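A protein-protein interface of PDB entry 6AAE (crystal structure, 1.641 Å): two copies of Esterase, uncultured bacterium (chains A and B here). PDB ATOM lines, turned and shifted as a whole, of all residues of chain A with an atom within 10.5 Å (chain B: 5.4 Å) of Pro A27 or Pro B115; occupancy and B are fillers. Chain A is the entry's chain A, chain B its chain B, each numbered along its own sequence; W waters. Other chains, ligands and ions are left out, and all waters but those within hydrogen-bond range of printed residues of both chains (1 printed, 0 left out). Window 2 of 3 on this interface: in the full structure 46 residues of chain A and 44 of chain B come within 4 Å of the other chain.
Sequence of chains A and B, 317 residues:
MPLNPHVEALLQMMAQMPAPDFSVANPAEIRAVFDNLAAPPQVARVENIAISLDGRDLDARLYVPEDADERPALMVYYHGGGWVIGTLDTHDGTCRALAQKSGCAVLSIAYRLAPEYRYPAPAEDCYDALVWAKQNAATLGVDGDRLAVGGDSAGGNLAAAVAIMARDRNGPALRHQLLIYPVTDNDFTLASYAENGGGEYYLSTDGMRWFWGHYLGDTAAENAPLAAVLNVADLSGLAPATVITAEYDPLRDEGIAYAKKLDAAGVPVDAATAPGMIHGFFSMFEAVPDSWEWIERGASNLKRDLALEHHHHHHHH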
ATOM      1  N   PHE A  22     -26.131   2.378 -26.995  1.00  0.00           N
ATOM      2  CA  PHE A  22     -26.629   2.679 -25.666  1.00  0.00           C
ATOM      3  C   PHE A  22     -28.159   2.555 -25.587  1.00  0.00           C
ATOM      4  O   PHE A  22     -28.892   2.857 -26.541  1.00  0.00           O
ATOM      5  CB  PHE A  22     -26.140   4.059 -25.228  1.00  0.00           C
ATOM      6  CG  PHE A  22     -24.681   4.060 -24.871  1.00  0.00           C
ATOM      7  CD1 PHE A  22     -24.238   3.305 -23.799  1.00  0.00           C
ATOM      8  CD2 PHE A  22     -23.750   4.787 -25.602  1.00  0.00           C
ATOM      9  CE1 PHE A  22     -22.896   3.266 -23.456  1.00  0.00           C
ATOM     10  CE2 PHE A  22     -22.400   4.756 -25.257  1.00  0.00           C
ATOM     11  CZ  PHE A  22     -21.978   3.995 -24.183  1.00  0.00           C
ATOM     12  N   SER A  23     -28.622   2.110 -24.423  1.00  0.00           N
ATOM     13  CA  SER A  23     -30.030   1.813 -24.183  1.00  0.00           C
ATOM     14  C   SER A  23     -30.829   3.078 -23.881  1.00  0.00           C
ATOM     15  O   SER A  23     -32.030   3.158 -24.165  1.00  0.00           O
ATOM     16  CB  SER A  23     -30.162   0.812 -23.022  1.00  0.00           C
ATOM     17  OG  SER A  23     -31.516   0.564 -22.693  1.00  0.00           O
ATOM     18  N   VAL A  24     -30.162   4.067 -23.293  1.00  0.00           N
ATOM     19  CA  VAL A  24     -30.855   5.281 -22.899  1.00  0.00           C
ATOM     20  C   VAL A  24     -29.937   6.509 -22.957  1.00  0.00           C
ATOM     21  O   VAL A  24     -28.718   6.415 -22.774  1.00  0.00           O
ATOM     22  CB  VAL A  24     -31.461   5.127 -21.475  1.00  0.00           C
ATOM     23  CG1 VAL A  24     -30.367   5.060 -20.430  1.00  0.00           C
ATOM     24  CG2 VAL A  24     -32.444   6.252 -21.160  1.00  0.00           C
ATOM     25  N   ALA A  25     -30.548   7.660 -23.223  1.00  0.00           N
ATOM     26  CA  ALA A  25     -29.833   8.929 -23.318  1.00  0.00           C
ATOM     27  C   ALA A  25     -29.698   9.593 -21.962  1.00  0.00           C
ATOM     28  O   ALA A  25     -30.456  10.501 -21.620  1.00  0.00           O
ATOM     29  CB  ALA A  25     -30.551   9.859 -24.295  1.00  0.00           C
ATOM     30  N   ASN A  26     -28.749   9.114 -21.167  1.00  0.00           N
ATOM     31  CA  ASN A  26     -28.371   9.802 -19.948  1.00  0.00           C
ATOM     32  C   ASN A  26     -27.015  10.483 -20.175  1.00  0.00           C
ATOM     33  O   ASN A  26     -26.344  10.177 -21.160  1.00  0.00           O
ATOM     34  CB  ASN A  26     -28.328   8.820 -18.777  1.00  0.00           C
ATOM     35  CG  ASN A  26     -29.693   8.614 -18.152  1.00  0.00           C
ATOM     36  OD1 ASN A  26     -30.489   9.546 -18.086  1.00  0.00           O
ATOM     37  ND2 ASN A  26     -29.964   7.390 -17.676  1.00  0.00           N
ATOM     38  N   PRO A  27     -26.613  11.392 -19.279  1.00  0.00           N
ATOM     39  CA  PRO A  27     -25.387  12.164 -19.543  1.00  0.00           C
ATOM     40  C   PRO A  27     -24.133  11.316 -19.788  1.00  0.00           C
ATOM     41  O   PRO A  27     -23.379  11.622 -20.710  1.00  0.00           O
ATOM     42  CB  PRO A  27     -25.241  13.006 -18.285  1.00  0.00           C
ATOM     43  CG  PRO A  27     -26.662  13.255 -17.861  1.00  0.00           C
ATOM     44  CD  PRO A  27     -27.373  11.950 -18.144  1.00  0.00           C
ATOM     45  N   ALA A  28     -23.913  10.258 -19.012  1.00  0.00           N
ATOM     46  CA  ALA A  28     -22.695   9.478 -19.190  1.00  0.00           C
ATOM     47  C   ALA A  28     -22.638   8.866 -20.593  1.00  0.00           C
ATOM     48  O   ALA A  28     -21.584   8.868 -21.233  1.00  0.00           O
ATOM     49  CB  ALA A  28     -22.586   8.380 -18.112  1.00  0.00           C
ATOM     50  N   GLU A  29     -23.774   8.374 -21.075  1.00  0.00           N
ATOM     51  CA  GLU A  29     -23.849   7.776 -22.405  1.00  0.00           C
ATOM     52  C   GLU A  29     -23.573   8.800 -23.504  1.00  0.00           C
ATOM     53  O   GLU A  29     -22.825   8.532 -24.454  1.00  0.00           O
ATOM     54  CB  GLU A  29     -25.228   7.157 -22.643  1.00  0.00           C
ATOM     55  CG  GLU A  29     -25.471   5.826 -21.945  1.00  0.00           C
ATOM     56  CD  GLU A  29     -25.843   5.948 -20.472  1.00  0.00           C
ATOM     57  OE1 GLU A  29     -25.815   7.065 -19.902  1.00  0.00           O
ATOM     58  OE2 GLU A  29     -26.178   4.899 -19.881  1.00  0.00           O
ATOM     59  N   ILE A  30     -24.208   9.958 -23.378  1.00  0.00           N
ATOM     60  CA  ILE A  30     -24.117  10.978 -24.418  1.00  0.00           C
ATOM     61  C   ILE A  30     -22.702  11.564 -24.410  1.00  0.00           C
ATOM     62  O   ILE A  30     -22.144  11.830 -25.467  1.00  0.00           O
ATOM     63  CB  ILE A  30     -25.179  12.065 -24.229  1.00  0.00           C
ATOM     64  CG1 ILE A  30     -26.581  11.444 -24.299  1.00  0.00           C
ATOM     65  CG2 ILE A  30     -25.039  13.172 -25.283  1.00  0.00           C
ATOM     66  CD1 ILE A  30     -26.827  10.650 -25.547  1.00  0.00           C
ATOM     67  N   ARG A  31     -22.125  11.740 -23.223  1.00  0.00           N
ATOM     68  CA  ARG A  31     -20.729  12.176 -23.101  1.00  0.00           C
ATOM     69  C   ARG A  31     -19.805  11.210 -23.822  1.00  0.00           C
ATOM     70  O   ARG A  31     -18.893  11.614 -24.543  1.00  0.00           O
ATOM     71  CB  ARG A  31     -20.313  12.293 -21.634  1.00  0.00           C
ATOM     72  CG  ARG A  31     -20.931  13.490 -20.945  1.00  0.00           C
ATOM     73  CD  ARG A  31     -20.726  13.478 -19.446  1.00  0.00           C
ATOM     74  NE  ARG A  31     -21.416  14.620 -18.868  1.00  0.00           N
ATOM     75  CZ  ARG A  31     -21.853  14.701 -17.619  1.00  0.00           C
ATOM     76  NH1 ARG A  31     -21.676  13.687 -16.769  1.00  0.00           N
ATOM     77  NH2 ARG A  31     -22.479  15.801 -17.228  1.00  0.00           N
ATOM     78  N   ALA A  32     -20.055   9.917 -23.624  1.00  0.00           N
ATOM     79  CA  ALA A  32     -19.213   8.883 -24.206  1.00  0.00           C
ATOM     80  C   ALA A  32     -19.299   8.902 -25.722  1.00  0.00           C
ATOM     81  O   ALA A  32     -18.276   8.827 -26.405  1.00  0.00           O
ATOM     82  CB  ALA A  32     -19.612   7.505 -23.664  1.00  0.00           C
ATOM     83  N   VAL A  33     -20.517   9.002 -26.247  1.00  0.00           N
ATOM     84  CA  VAL A  33     -20.713   9.070 -27.694  1.00  0.00           C
ATOM     85  C   VAL A  33     -20.002  10.293 -28.290  1.00  0.00           C
ATOM     86  O   VAL A  33     -19.302  10.179 -29.297  1.00  0.00           O
ATOM     87  CB  VAL A  33     -22.199   9.123 -28.054  1.00  0.00           C
ATOM     88  CG1 VAL A  33     -22.378   9.360 -29.540  1.00  0.00           C
ATOM     89  CG2 VAL A  33     -22.887   7.832 -27.630  1.00  0.00           C
ATOM     90  N   PHE A  34     -20.164  11.451 -27.652  1.00  0.00           N
ATOM     91  CA  PHE A  34     -19.562  12.681 -28.162  1.00  0.00           C
ATOM     92  C   PHE A  34     -18.032  12.632 -28.070  1.00  0.00           C
ATOM     93  O   PHE A  34     -17.347  13.038 -29.007  1.00  0.00           O
ATOM     94  CB  PHE A  34     -20.099  13.902 -27.413  1.00  0.00           C
ATOM     95  CG  PHE A  34     -19.656  15.209 -28.006  1.00  0.00           C
ATOM     96  CD1 PHE A  34     -19.978  15.528 -29.317  1.00  0.00           C
ATOM     97  CD2 PHE A  34     -18.926  16.117 -27.251  1.00  0.00           C
ATOM     98  CE1 PHE A  34     -19.579  16.726 -29.870  1.00  0.00           C
ATOM     99  CE2 PHE A  34     -18.517  17.320 -27.798  1.00  0.00           C
ATOM    100  CZ  PHE A  34     -18.848  17.623 -29.115  1.00  0.00           C
ATOM    101  N   ASP A  35     -17.493  12.140 -26.957  1.00  0.00           N
ATOM    102  CA  ASP A  35     -16.042  11.924 -26.859  1.00  0.00           C
ATOM    103  C   ASP A  35     -15.502  11.043 -27.988  1.00  0.00           C
ATOM    104  O   ASP A  35     -14.450  11.324 -28.570  1.00  0.00           O
ATOM    105  CB  ASP A  35     -15.673  11.282 -25.527  1.00  0.00           C
ATOM    106  CG  ASP A  35     -15.883  12.211 -24.354  1.00  0.00           C
ATOM    107  OD1 ASP A  35     -15.995  13.431 -24.580  1.00  0.00           O
ATOM    108  OD2 ASP A  35     -15.935  11.722 -23.204  1.00  0.00           O
ATOM    109  N   VAL B  84     -23.767  20.082 -20.930  1.00  0.00           N
ATOM    110  CA  VAL B  84     -23.805  18.739 -20.344  1.00  0.00           C
ATOM    111  C   VAL B  84     -22.611  17.882 -20.775  1.00  0.00           C
ATOM    112  O   VAL B  84     -22.113  17.057 -19.996  1.00  0.00           O
ATOM    113  CB  VAL B  84     -25.105  18.010 -20.735  1.00  0.00           C
ATOM    114  CG1 VAL B  84     -25.111  16.589 -20.168  1.00  0.00           C
ATOM    115  CG2 VAL B  84     -26.324  18.773 -20.221  1.00  0.00           C
ATOM    116  N   ILE B  85     -22.144  18.092 -22.010  1.00  0.00           N
ATOM    117  CA  ILE B  85     -21.068  17.275 -22.583  1.00  0.00           C
ATOM    118  C   ILE B  85     -19.936  18.152 -23.119  1.00  0.00           C
ATOM    119  O   ILE B  85     -19.992  19.365 -22.995  1.00  0.00           O
ATOM    120  CB  ILE B  85     -21.574  16.337 -23.705  1.00  0.00           C
ATOM    121  CG1 ILE B  85     -21.984  17.096 -24.962  1.00  0.00           C
ATOM    122  CG2 ILE B  85     -22.803  15.518 -23.221  1.00  0.00           C
ATOM    123  CD1 ILE B  85     -22.659  16.232 -26.020  1.00  0.00           C
ATOM    124  N   LEU B 113     -20.130  20.751 -15.414  1.00  0.00           N
ATOM    125  CA  LEU B 113     -21.240  20.446 -16.325  1.00  0.00           C
ATOM    126  C   LEU B 113     -22.521  20.064 -15.606  1.00  0.00           C
ATOM    127  O   LEU B 113     -22.490  19.542 -14.502  1.00  0.00           O
ATOM    128  CB  LEU B 113     -20.856  19.304 -17.272  1.00  0.00           C
ATOM    129  CG  LEU B 113     -19.646  19.608 -18.164  1.00  0.00           C
ATOM    130  CD1 LEU B 113     -19.117  18.351 -18.810  1.00  0.00           C
ATOM    131  CD2 LEU B 113     -20.079  20.613 -19.238  1.00  0.00           C
ATOM    132  N   ALA B 114     -23.642  20.332 -16.260  1.00  0.00           N
ATOM    133  CA  ALA B 114     -24.949  19.895 -15.794  1.00  0.00           C
ATOM    134  C   ALA B 114     -25.154  18.449 -16.231  1.00  0.00           C
ATOM    135  O   ALA B 114     -24.520  17.987 -17.183  1.00  0.00           O
ATOM    136  CB  ALA B 114     -26.039  20.810 -16.366  1.00  0.00           C
ATOM    137  N   PRO B 115     -26.066  17.710 -15.571  1.00  0.00           N
ATOM    138  CA  PRO B 115     -26.971  18.068 -14.471  1.00  0.00           C
ATOM    139  C   PRO B 115     -26.317  18.035 -13.098  1.00  0.00           C
ATOM    140  O   PRO B 115     -26.944  18.464 -12.121  1.00  0.00           O
ATOM    141  CB  PRO B 115     -28.066  17.004 -14.566  1.00  0.00           C
ATOM    142  CG  PRO B 115     -27.365  15.803 -15.155  1.00  0.00           C
ATOM    143  CD  PRO B 115     -26.371  16.387 -16.137  1.00  0.00           C
ATOM    144  N   GLU B 116     -25.081  17.555 -13.019  1.00  0.00           N
ATOM    145  CA  GLU B 116     -24.358  17.548 -11.754  1.00  0.00           C
ATOM    146  C   GLU B 116     -24.262  18.953 -11.174  1.00  0.00           C
ATOM    147  O   GLU B 116     -24.479  19.157  -9.970  1.00  0.00           O
ATOM    148  CB  GLU B 116     -22.953  16.952 -11.933  1.00  0.00           C
ATOM    149  CG  GLU B 116     -22.913  15.459 -12.219  1.00  0.00           C
ATOM    150  CD  GLU B 116     -22.917  15.120 -13.708  1.00  0.00           C
ATOM    151  OE1 GLU B 116     -23.316  15.973 -14.526  1.00  0.00           O
ATOM    152  OE2 GLU B 116     -22.556  13.979 -14.063  1.00  0.00           O
ATOM    153  N   TYR B 117     -23.940  19.921 -12.038  1.00  0.00           N
ATOM    154  CA  TYR B 117     -23.852  21.321 -11.638  1.00  0.00           C
ATOM    155  C   TYR B 117     -24.814  22.126 -12.491  1.00  0.00           C
ATOM    156  O   TYR B 117     -24.525  22.457 -13.640  1.00  0.00           O
ATOM    157  CB  TYR B 117     -22.411  21.836 -11.767  1.00  0.00           C
ATOM    158  CG  TYR B 117     -21.506  21.063 -10.850  1.00  0.00           C
ATOM    159  CD1 TYR B 117     -21.356  21.439  -9.523  1.00  0.00           C
ATOM    160  CD2 TYR B 117     -20.883  19.908 -11.285  1.00  0.00           C
ATOM    161  CE1 TYR B 117     -20.571  20.706  -8.663  1.00  0.00           C
ATOM    162  CE2 TYR B 117     -20.094  19.164 -10.433  1.00  0.00           C
ATOM    163  CZ  TYR B 117     -19.946  19.566  -9.126  1.00  0.00           C
ATOM    164  OH  TYR B 117     -19.165  18.825  -8.275  1.00  0.00           O
ATOM    165  N   ARG B 118     -25.982  22.420 -11.933  1.00  0.00           N
ATOM    166  CA  ARG B 118     -27.005  23.093 -12.713  1.00  0.00           C
ATOM    167  C   ARG B 118     -26.769  24.589 -12.752  1.00  0.00           C
ATOM    168  O   ARG B 118     -25.968  25.117 -11.968  1.00  0.00           O
ATOM    169  CB  ARG B 118     -28.385  22.781 -12.146  1.00  0.00           C
ATOM    170  CG  ARG B 118     -28.671  21.279 -12.143  1.00  0.00           C
ATOM    171  CD  ARG B 118     -30.135  21.007 -12.126  1.00  0.00           C
ATOM    172  NE  ARG B 118     -30.443  19.628 -11.769  1.00  0.00           N
ATOM    173  CZ  ARG B 118     -30.875  18.708 -12.624  1.00  0.00           C
ATOM    174  NH1 ARG B 118     -31.033  18.998 -13.908  1.00  0.00           N
ATOM    175  NH2 ARG B 118     -31.154  17.488 -12.188  1.00  0.00           N
ATOM    176  N   TRP B 210     -33.553  18.341 -24.190  1.00  0.00           N
ATOM    177  CA  TRP B 210     -32.769  17.520 -23.258  1.00  0.00           C
ATOM    178  C   TRP B 210     -31.669  18.319 -22.562  1.00  0.00           C
ATOM    179  O   TRP B 210     -31.549  18.299 -21.343  1.00  0.00           O
ATOM    180  CB  TRP B 210     -32.166  16.352 -24.029  1.00  0.00           C
ATOM    181  CG  TRP B 210     -31.495  15.257 -23.237  1.00  0.00           C
ATOM    182  CD1 TRP B 210     -32.082  14.135 -22.722  1.00  0.00           C
ATOM    183  CD2 TRP B 210     -30.092  15.144 -22.948  1.00  0.00           C
ATOM    184  NE1 TRP B 210     -31.137  13.343 -22.109  1.00  0.00           N
ATOM    185  CE2 TRP B 210     -29.905  13.939 -22.239  1.00  0.00           C
ATOM    186  CE3 TRP B 210     -28.976  15.946 -23.223  1.00  0.00           C
ATOM    187  CZ2 TRP B 210     -28.647  13.523 -21.788  1.00  0.00           C
ATOM    188  CZ3 TRP B 210     -27.733  15.533 -22.780  1.00  0.00           C
ATOM    189  CH2 TRP B 210     -27.577  14.330 -22.062  1.00  0.00           C
ATOM    190  N   HIS B 214     -31.556  19.502 -18.473  1.00  0.00           N
ATOM    191  CA  HIS B 214     -30.463  19.217 -17.548  1.00  0.00           C
ATOM    192  C   HIS B 214     -29.831  20.485 -16.965  1.00  0.00           C
ATOM    193  O   HIS B 214     -29.467  20.527 -15.799  1.00  0.00           O
ATOM    194  CB  HIS B 214     -29.389  18.371 -18.242  1.00  0.00           C
ATOM    195  CG  HIS B 214     -29.760  16.928 -18.375  1.00  0.00           C
ATOM    196  ND1 HIS B 214     -30.187  16.175 -17.303  1.00  0.00           N
ATOM    197  CD2 HIS B 214     -29.762  16.100 -19.443  1.00  0.00           C
ATOM    198  CE1 HIS B 214     -30.444  14.946 -17.708  1.00  0.00           C
ATOM    199  NE2 HIS B 214     -30.193  14.872 -19.001  1.00  0.00           N
HETATM  200  O   HOH W   1     -31.192  12.165 -19.046  1.00  0.00           O
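OE1 of Glu B116 lies within salt-bridge range of NH2 of Arg A31, 2.8 Å away. The guanidinium group (NE) of Arg A31 sits at hydrogen-bond distance from the backbone carbonyl oxygen (O) of Val B84 (2.8 Å). NH2 of Arg A31 is in hydrogen-bond range of O of Ala B114, at 3.0 Å. NE1 of Trp B210 is in hydrogen-bond range of O of Ala A25 (3.0 Å).
Among the printed residues, merely in contact across the chains: Asn A26 with Trp B210 (3.8 Å), Pro A27 with Pro B115 (3.6 Å), Pro A27 with Trp B210 (3.9 Å), Ile A30 with Ile B85 (3.8 Å), Ile A30 with Trp B210 (3.8 Å), Arg A31 with Ile B85 (3.6 Å), Arg A31 with Leu B113 (3.9 Å) and Phe A34 with Ile B85 (3.7 Å).
Of the printed residues of chain B, Ala A25 touches Trp B210. Of chain B, only Pro B115 (3.6 Å) and Trp B210 (3.9 Å) come within 4 Å of Pro A27. Ala A32 touches none of the printed residues of chain B. Printed residues of chain A within 4 Å of Val B84: Arg A31. Of the printed residues of chain A, Leu B113 touches Arg A31 (3.9 Å). Ala B114 touches just one residue of chain A: Arg A31. No residue of chain A comes within 4 Å of His B214. The nearest printed residue of chain B that does not touch Pro A27 is His B214 (4.05 Å). The nearest residue of chain A that does not touch Pro B115 is Arg A31 (4.1 Å). The nearest printed residue of chain A that does not touch Leu B113 is Pro A27 (7.7 Å).
Printed residues of chain A that touch a printed residue of chain B: Ala A25, Asn A26, Pro A27, Ile A30, Arg A31 and Phe A34. Along chain A the printed residues that touch a printed residue of chain B span positions 25 to 34. Hydrophobic or aromatic side chains of chain B within 4 Å of the printed part of chain A: Ile B85, Leu B113, Pro B115 and Trp B210. Along chain B the printed residues that touch a printed residue of chain A span positions 84 to 210. Among the printed residues, 12 pairs touch across the chains. Among the printed residues, Asp or Glu carboxylates within 4 Å of a Lys or Arg side-chain nitrogen of the other chain: Arg A31 with Glu B116.
No position is printed for both chains. Of the 12 pairs that touch across the chains among the printed residues, none has its exchanged pair printed and touching as well.
Water W1 lies within hydrogen-bond range of OD1 of Asn A26, NE2 of His B214, O of Ala A25 and NE1 of Trp B210.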
